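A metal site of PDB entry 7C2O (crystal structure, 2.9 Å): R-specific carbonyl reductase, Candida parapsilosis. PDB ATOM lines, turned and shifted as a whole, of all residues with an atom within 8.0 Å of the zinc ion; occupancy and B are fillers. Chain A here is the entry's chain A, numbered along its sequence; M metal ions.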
ATOM      1  N   SER A 100      26.533 -33.538 -21.083  1.00  0.00           N
ATOM      2  CA  SER A 100      27.068 -32.456 -20.268  1.00  0.00           C
ATOM      3  C   SER A 100      26.892 -31.142 -21.020  1.00  0.00           C
ATOM      4  O   SER A 100      26.535 -31.109 -22.203  1.00  0.00           O
ATOM      5  CB  SER A 100      28.539 -32.699 -19.901  1.00  0.00           C
ATOM      6  OG  SER A 100      29.362 -32.682 -21.061  1.00  0.00           O
ATOM      7  N   SER A 101      27.130 -30.050 -20.306  1.00  0.00           N
ATOM      8  CA  SER A 101      27.047 -28.708 -20.868  1.00  0.00           C
ATOM      9  C   SER A 101      27.915 -27.786 -20.020  1.00  0.00           C
ATOM     10  O   SER A 101      28.488 -28.197 -19.006  1.00  0.00           O
ATOM     11  CB  SER A 101      25.603 -28.222 -20.945  1.00  0.00           C
ATOM     12  OG  SER A 101      25.044 -28.063 -19.651  1.00  0.00           O
ATOM     13  N   CYS A 102      28.007 -26.517 -20.435  1.00  0.00           N
ATOM     14  CA  CYS A 102      28.962 -25.599 -19.807  1.00  0.00           C
ATOM     15  C   CYS A 102      28.548 -25.217 -18.397  1.00  0.00           C
ATOM     16  O   CYS A 102      29.415 -24.845 -17.594  1.00  0.00           O
ATOM     17  CB  CYS A 102      29.127 -24.343 -20.673  1.00  0.00           C
ATOM     18  SG  CYS A 102      27.973 -23.006 -20.310  1.00  0.00           S
ATOM     19  N   ARG A 103      27.256 -25.288 -18.075  1.00  0.00           N
ATOM     20  CA  ARG A 103      26.720 -24.898 -16.761  1.00  0.00           C
ATOM     21  C   ARG A 103      26.991 -23.434 -16.437  1.00  0.00           C
ATOM     22  O   ARG A 103      26.945 -23.039 -15.270  1.00  0.00           O
ATOM     23  CB  ARG A 103      27.270 -25.792 -15.641  1.00  0.00           C
ATOM     24  CG  ARG A 103      26.494 -27.076 -15.421  1.00  0.00           C
ATOM     25  CD  ARG A 103      27.080 -27.910 -14.284  1.00  0.00           C
ATOM     26  NE  ARG A 103      26.192 -29.026 -13.937  1.00  0.00           N
ATOM     27  CZ  ARG A 103      25.285 -28.979 -12.970  1.00  0.00           C
ATOM     28  NH1 ARG A 103      25.142 -27.878 -12.240  1.00  0.00           N
ATOM     29  NH2 ARG A 103      24.519 -30.035 -12.723  1.00  0.00           N
ATOM     30  N   SER A 104      27.278 -22.616 -17.449  1.00  0.00           N
ATOM     31  CA  SER A 104      27.543 -21.207 -17.238  1.00  0.00           C
ATOM     32  C   SER A 104      26.953 -20.311 -18.314  1.00  0.00           C
ATOM     33  O   SER A 104      27.198 -19.100 -18.283  1.00  0.00           O
ATOM     34  CB  SER A 104      29.047 -20.945 -17.126  1.00  0.00           C
ATOM     35  OG  SER A 104      29.705 -21.263 -18.341  1.00  0.00           O
ATOM     36  N   CYS A 105      26.215 -20.855 -19.283  1.00  0.00           N
ATOM     37  CA  CYS A 105      25.616 -20.028 -20.311  1.00  0.00           C
ATOM     38  C   CYS A 105      24.200 -19.635 -19.879  1.00  0.00           C
ATOM     39  O   CYS A 105      23.696 -20.054 -18.840  1.00  0.00           O
ATOM     40  CB  CYS A 105      25.591 -20.777 -21.640  1.00  0.00           C
ATOM     41  SG  CYS A 105      24.379 -22.089 -21.731  1.00  0.00           S
ATOM     42  N   GLN A 106      23.559 -18.798 -20.707  1.00  0.00           N
ATOM     43  CA  GLN A 106      22.157 -18.486 -20.481  1.00  0.00           C
ATOM     44  C   GLN A 106      21.254 -19.646 -20.888  1.00  0.00           C
ATOM     45  O   GLN A 106      20.192 -19.826 -20.287  1.00  0.00           O
ATOM     46  CB  GLN A 106      21.789 -17.201 -21.235  1.00  0.00           C
ATOM     47  CG  GLN A 106      20.333 -16.777 -21.107  1.00  0.00           C
ATOM     48  CD  GLN A 106      20.068 -15.928 -19.863  1.00  0.00           C
ATOM     49  OE1 GLN A 106      20.747 -16.062 -18.846  1.00  0.00           O
ATOM     50  NE2 GLN A 106      19.089 -15.033 -19.956  1.00  0.00           N
ATOM     51  N   ARG A 107      21.669 -20.433 -21.875  1.00  0.00           N
ATOM     52  CA  ARG A 107      20.846 -21.551 -22.331  1.00  0.00           C
ATOM     53  C   ARG A 107      20.749 -22.641 -21.271  1.00  0.00           C
ATOM     54  O   ARG A 107      19.705 -23.296 -21.153  1.00  0.00           O
ATOM     55  CB  ARG A 107      21.405 -22.123 -23.637  1.00  0.00           C
ATOM     56  CG  ARG A 107      21.560 -21.078 -24.724  1.00  0.00           C
ATOM     57  CD  ARG A 107      22.055 -21.685 -26.017  1.00  0.00           C
ATOM     58  NE  ARG A 107      21.926 -20.768 -27.151  1.00  0.00           N
ATOM     59  CZ  ARG A 107      22.194 -21.089 -28.405  1.00  0.00           C
ATOM     60  NH1 ARG A 107      22.600 -22.308 -28.718  1.00  0.00           N
ATOM     61  NH2 ARG A 107      22.040 -20.188 -29.371  1.00  0.00           N
ATOM     62  N   CYS A 108      21.817 -22.851 -20.496  1.00  0.00           N
ATOM     63  CA  CYS A 108      21.800 -23.846 -19.435  1.00  0.00           C
ATOM     64  C   CYS A 108      20.825 -23.479 -18.319  1.00  0.00           C
ATOM     65  O   CYS A 108      20.349 -24.374 -17.615  1.00  0.00           O
ATOM     66  CB  CYS A 108      23.204 -24.002 -18.851  1.00  0.00           C
ATOM     67  SG  CYS A 108      24.298 -25.108 -19.779  1.00  0.00           S
ATOM     68  N   ASP A 109      20.549 -22.193 -18.145  1.00  0.00           N
ATOM     69  CA  ASP A 109      19.612 -21.720 -17.127  1.00  0.00           C
ATOM     70  C   ASP A 109      18.245 -21.380 -17.706  1.00  0.00           C
ATOM     71  O   ASP A 109      17.334 -21.051 -16.944  1.00  0.00           O
ATOM     72  CB  ASP A 109      20.195 -20.489 -16.414  1.00  0.00           C
ATOM     73  CG  ASP A 109      19.653 -20.316 -15.001  1.00  0.00           C
ATOM     74  OD1 ASP A 109      19.062 -21.281 -14.477  1.00  0.00           O
ATOM     75  OD2 ASP A 109      19.810 -19.216 -14.437  1.00  0.00           O
ATOM     76  N   ASN A 112      17.485 -24.747 -22.030  1.00  0.00           N
ATOM     77  CA  ASN A 112      18.011 -25.004 -23.356  1.00  0.00           C
ATOM     78  C   ASN A 112      19.428 -25.571 -23.287  1.00  0.00           C
ATOM     79  O   ASN A 112      20.258 -25.302 -24.159  1.00  0.00           O
ATOM     80  CB  ASN A 112      18.002 -23.737 -24.214  1.00  0.00           C
ATOM     81  CG  ASN A 112      16.746 -23.626 -25.064  1.00  0.00           C
ATOM     82  OD1 ASN A 112      16.195 -24.631 -25.509  1.00  0.00           O
ATOM     83  ND2 ASN A 112      16.288 -22.392 -25.286  1.00  0.00           N
ATOM     84  N   GLU A 113      19.717 -26.355 -22.245  1.00  0.00           N
ATOM     85  CA  GLU A 113      21.053 -26.895 -22.034  1.00  0.00           C
ATOM     86  C   GLU A 113      21.490 -27.823 -23.162  1.00  0.00           C
ATOM     87  O   GLU A 113      22.697 -28.050 -23.342  1.00  0.00           O
ATOM     88  CB  GLU A 113      21.117 -27.642 -20.701  1.00  0.00           C
ATOM     89  CG  GLU A 113      20.133 -28.792 -20.576  1.00  0.00           C
ATOM     90  CD  GLU A 113      18.750 -28.344 -20.160  1.00  0.00           C
ATOM     91  OE1 GLU A 113      17.836 -29.187 -20.107  1.00  0.00           O
ATOM     92  OE2 GLU A 113      18.569 -27.137 -19.896  1.00  0.00           O
ATOM     93  N   GLN A 114      20.537 -28.376 -23.929  1.00  0.00           N
ATOM     94  CA  GLN A 114      20.904 -29.194 -25.075  1.00  0.00           C
ATOM     95  C   GLN A 114      21.502 -28.382 -26.210  1.00  0.00           C
ATOM     96  O   GLN A 114      22.202 -28.942 -27.062  1.00  0.00           O
ATOM     97  CB  GLN A 114      19.674 -29.972 -25.572  1.00  0.00           C
ATOM     98  CG  GLN A 114      18.612 -29.098 -26.243  1.00  0.00           C
ATOM     99  CD  GLN A 114      17.684 -28.431 -25.235  1.00  0.00           C
ATOM    100  OE1 GLN A 114      18.019 -28.291 -24.060  1.00  0.00           O
ATOM    101  NE2 GLN A 114      16.516 -28.017 -25.700  1.00  0.00           N
ATOM    102  N   TYR A 115      21.246 -27.066 -26.233  1.00  0.00           N
ATOM    103  CA  TYR A 115      21.796 -26.174 -27.242  1.00  0.00           C
ATOM    104  C   TYR A 115      23.025 -25.417 -26.738  1.00  0.00           C
ATOM    105  O   TYR A 115      23.379 -24.386 -27.311  1.00  0.00           O
ATOM    106  CB  TYR A 115      20.730 -25.188 -27.710  1.00  0.00           C
ATOM    107  CG  TYR A 115      19.654 -25.816 -28.566  1.00  0.00           C
ATOM    108  CD1 TYR A 115      19.905 -26.158 -29.889  1.00  0.00           C
ATOM    109  CD2 TYR A 115      18.378 -26.054 -28.059  1.00  0.00           C
ATOM    110  CE1 TYR A 115      18.927 -26.719 -30.682  1.00  0.00           C
ATOM    111  CE2 TYR A 115      17.388 -26.617 -28.845  1.00  0.00           C
ATOM    112  CZ  TYR A 115      17.667 -26.950 -30.151  1.00  0.00           C
ATOM    113  OH  TYR A 115      16.687 -27.513 -30.935  1.00  0.00           O
ATOM    114  N   CYS A 116      23.665 -25.911 -25.692  1.00  0.00           N
ATOM    115  CA  CYS A 116      24.874 -25.277 -25.180  1.00  0.00           C
ATOM    116  C   CYS A 116      25.988 -25.367 -26.205  1.00  0.00           C
ATOM    117  O   CYS A 116      26.232 -26.434 -26.785  1.00  0.00           O
ATOM    118  CB  CYS A 116      25.297 -25.923 -23.862  1.00  0.00           C
ATOM    119  SG  CYS A 116      26.891 -25.358 -23.230  1.00  0.00           S
ATOM    120  N   LYS A 117      26.686 -24.248 -26.425  1.00  0.00           N
ATOM    121  CA  LYS A 117      27.733 -24.201 -27.432  1.00  0.00           C
ATOM    122  C   LYS A 117      28.858 -25.174 -27.104  1.00  0.00           C
ATOM    123  O   LYS A 117      29.426 -25.794 -28.003  1.00  0.00           O
ATOM    124  CB  LYS A 117      28.262 -22.771 -27.555  1.00  0.00           C
ATOM    125  CG  LYS A 117      29.337 -22.584 -28.617  1.00  0.00           C
ATOM    126  CD  LYS A 117      29.743 -21.119 -28.740  1.00  0.00           C
ATOM    127  CE  LYS A 117      30.121 -20.539 -27.375  1.00  0.00           C
ATOM    128  NZ  LYS A 117      30.549 -19.110 -27.458  1.00  0.00           N
ATOM    129  N   GLN A 118      29.177 -25.324 -25.823  1.00  0.00           N
ATOM    130  CA  GLN A 118      30.216 -26.236 -25.379  1.00  0.00           C
ATOM    131  C   GLN A 118      29.650 -27.570 -24.887  1.00  0.00           C
ATOM    132  O   GLN A 118      30.320 -28.266 -24.114  1.00  0.00           O
ATOM    133  CB  GLN A 118      31.069 -25.583 -24.287  1.00  0.00           C
ATOM    134  CG  GLN A 118      31.895 -24.408 -24.782  1.00  0.00           C
ATOM    135  CD  GLN A 118      32.672 -23.741 -23.672  1.00  0.00           C
ATOM    136  OE1 GLN A 118      32.337 -23.868 -22.491  1.00  0.00           O
ATOM    137  NE2 GLN A 118      33.737 -23.027 -24.045  1.00  0.00           N
ATOM    138  N   GLY A 119      28.452 -27.930 -25.333  1.00  0.00           N
ATOM    139  CA  GLY A 119      27.873 -29.200 -24.936  1.00  0.00           C
ATOM    140  C   GLY A 119      28.623 -30.371 -25.532  1.00  0.00           C
ATOM    141  O   GLY A 119      29.350 -30.250 -26.531  1.00  0.00           O
ATOM    142  N   ARG A 129      35.123 -30.403 -20.486  1.00  0.00           N
ATOM    143  CA  ARG A 129      35.137 -30.371 -19.033  1.00  0.00           C
ATOM    144  C   ARG A 129      35.770 -31.611 -18.424  1.00  0.00           C
ATOM    145  O   ARG A 129      35.862 -31.704 -17.191  1.00  0.00           O
ATOM    146  CB  ARG A 129      33.713 -30.206 -18.494  1.00  0.00           C
ATOM    147  CG  ARG A 129      33.125 -28.834 -18.742  1.00  0.00           C
ATOM    148  CD  ARG A 129      31.617 -28.850 -18.662  1.00  0.00           C
ATOM    149  NE  ARG A 129      31.015 -29.774 -19.610  1.00  0.00           N
ATOM    150  CZ  ARG A 129      30.840 -29.526 -20.898  1.00  0.00           C
ATOM    151  NH1 ARG A 129      31.238 -28.361 -21.400  1.00  0.00           N
ATOM    152  NH2 ARG A 129      30.286 -30.430 -21.689  1.00  0.00           N
ATOM    153  N   LYS A 148      22.343 -32.762 -14.966  1.00  0.00           N
ATOM    154  CA  LYS A 148      21.356 -32.011 -15.744  1.00  0.00           C
ATOM    155  C   LYS A 148      20.891 -32.777 -16.970  1.00  0.00           C
ATOM    156  O   LYS A 148      19.851 -32.431 -17.553  1.00  0.00           O
ATOM    157  CB  LYS A 148      21.934 -30.649 -16.147  1.00  0.00           C
ATOM    158  CG  LYS A 148      20.936 -29.718 -16.837  1.00  0.00           C
ATOM    159  CD  LYS A 148      21.473 -28.316 -17.047  1.00  0.00           C
ATOM    160  CE  LYS A 148      22.455 -27.907 -15.966  1.00  0.00           C
ATOM    161  NZ  LYS A 148      22.525 -26.422 -15.855  1.00  0.00           N
ATOM    162  N   PHE A 149      21.605 -33.828 -17.358  1.00  0.00           N
ATOM    163  CA  PHE A 149      21.215 -34.654 -18.496  1.00  0.00           C
ATOM    164  C   PHE A 149      20.820 -36.069 -18.084  1.00  0.00           C
ATOM    165  O   PHE A 149      20.608 -36.915 -18.951  1.00  0.00           O
ATOM    166  CB  PHE A 149      22.340 -34.681 -19.529  1.00  0.00           C
ATOM    167  CG  PHE A 149      22.599 -33.341 -20.166  1.00  0.00           C
ATOM    168  CD1 PHE A 149      21.909 -32.968 -21.303  1.00  0.00           C
ATOM    169  CD2 PHE A 149      23.497 -32.447 -19.606  1.00  0.00           C
ATOM    170  CE1 PHE A 149      22.121 -31.738 -21.895  1.00  0.00           C
ATOM    171  CE2 PHE A 149      23.716 -31.219 -20.186  1.00  0.00           C
ATOM    172  CZ  PHE A 149      23.027 -30.855 -21.324  1.00  0.00           C
HETATM  173 ZN    ZN M   1      26.043 -23.857 -21.313  1.00  0.00          ZN
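N of Gln 118 sits close to SG of Cys 116, 3.5 Å away.
The backbone NH (N) of Arg 103 lies close to the side-chain sulfur (SG) of Cys 108 (3.4 Å).
N of Gly 119 sits close to SG of Cys 116, at 3.7 Å.
SG of Cys 102 sits close to N of Ser 104 (3.0 Å).
The side-chain amino group of Lys 148 sits at hydrogen-bond distance from the backbone carbonyl oxygen of Cys 108, at 3.5 Å.
The side-chain sulfur of Cys 108 lies close to the side-chain hydroxyl of Ser 101 (3.1 Å).
SG of Cys 105 lies close to N of Arg 107, at 3.2 Å.
The zinc ion is bound by SG of Cys 102 (2.3 Å), SG of Cys 105 (2.5 Å), SG of Cys 116 (2.6 Å) and SG of Cys 108 (2.6 Å).
The zinc ion has four donor atoms within binding distance.
Residues that only touch the zinc ion: Arg 103.
Five residues have an atom within 4 Å of the zinc ion: Cys 102, Arg 103, Cys 105, Cys 108 and Cys 116.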
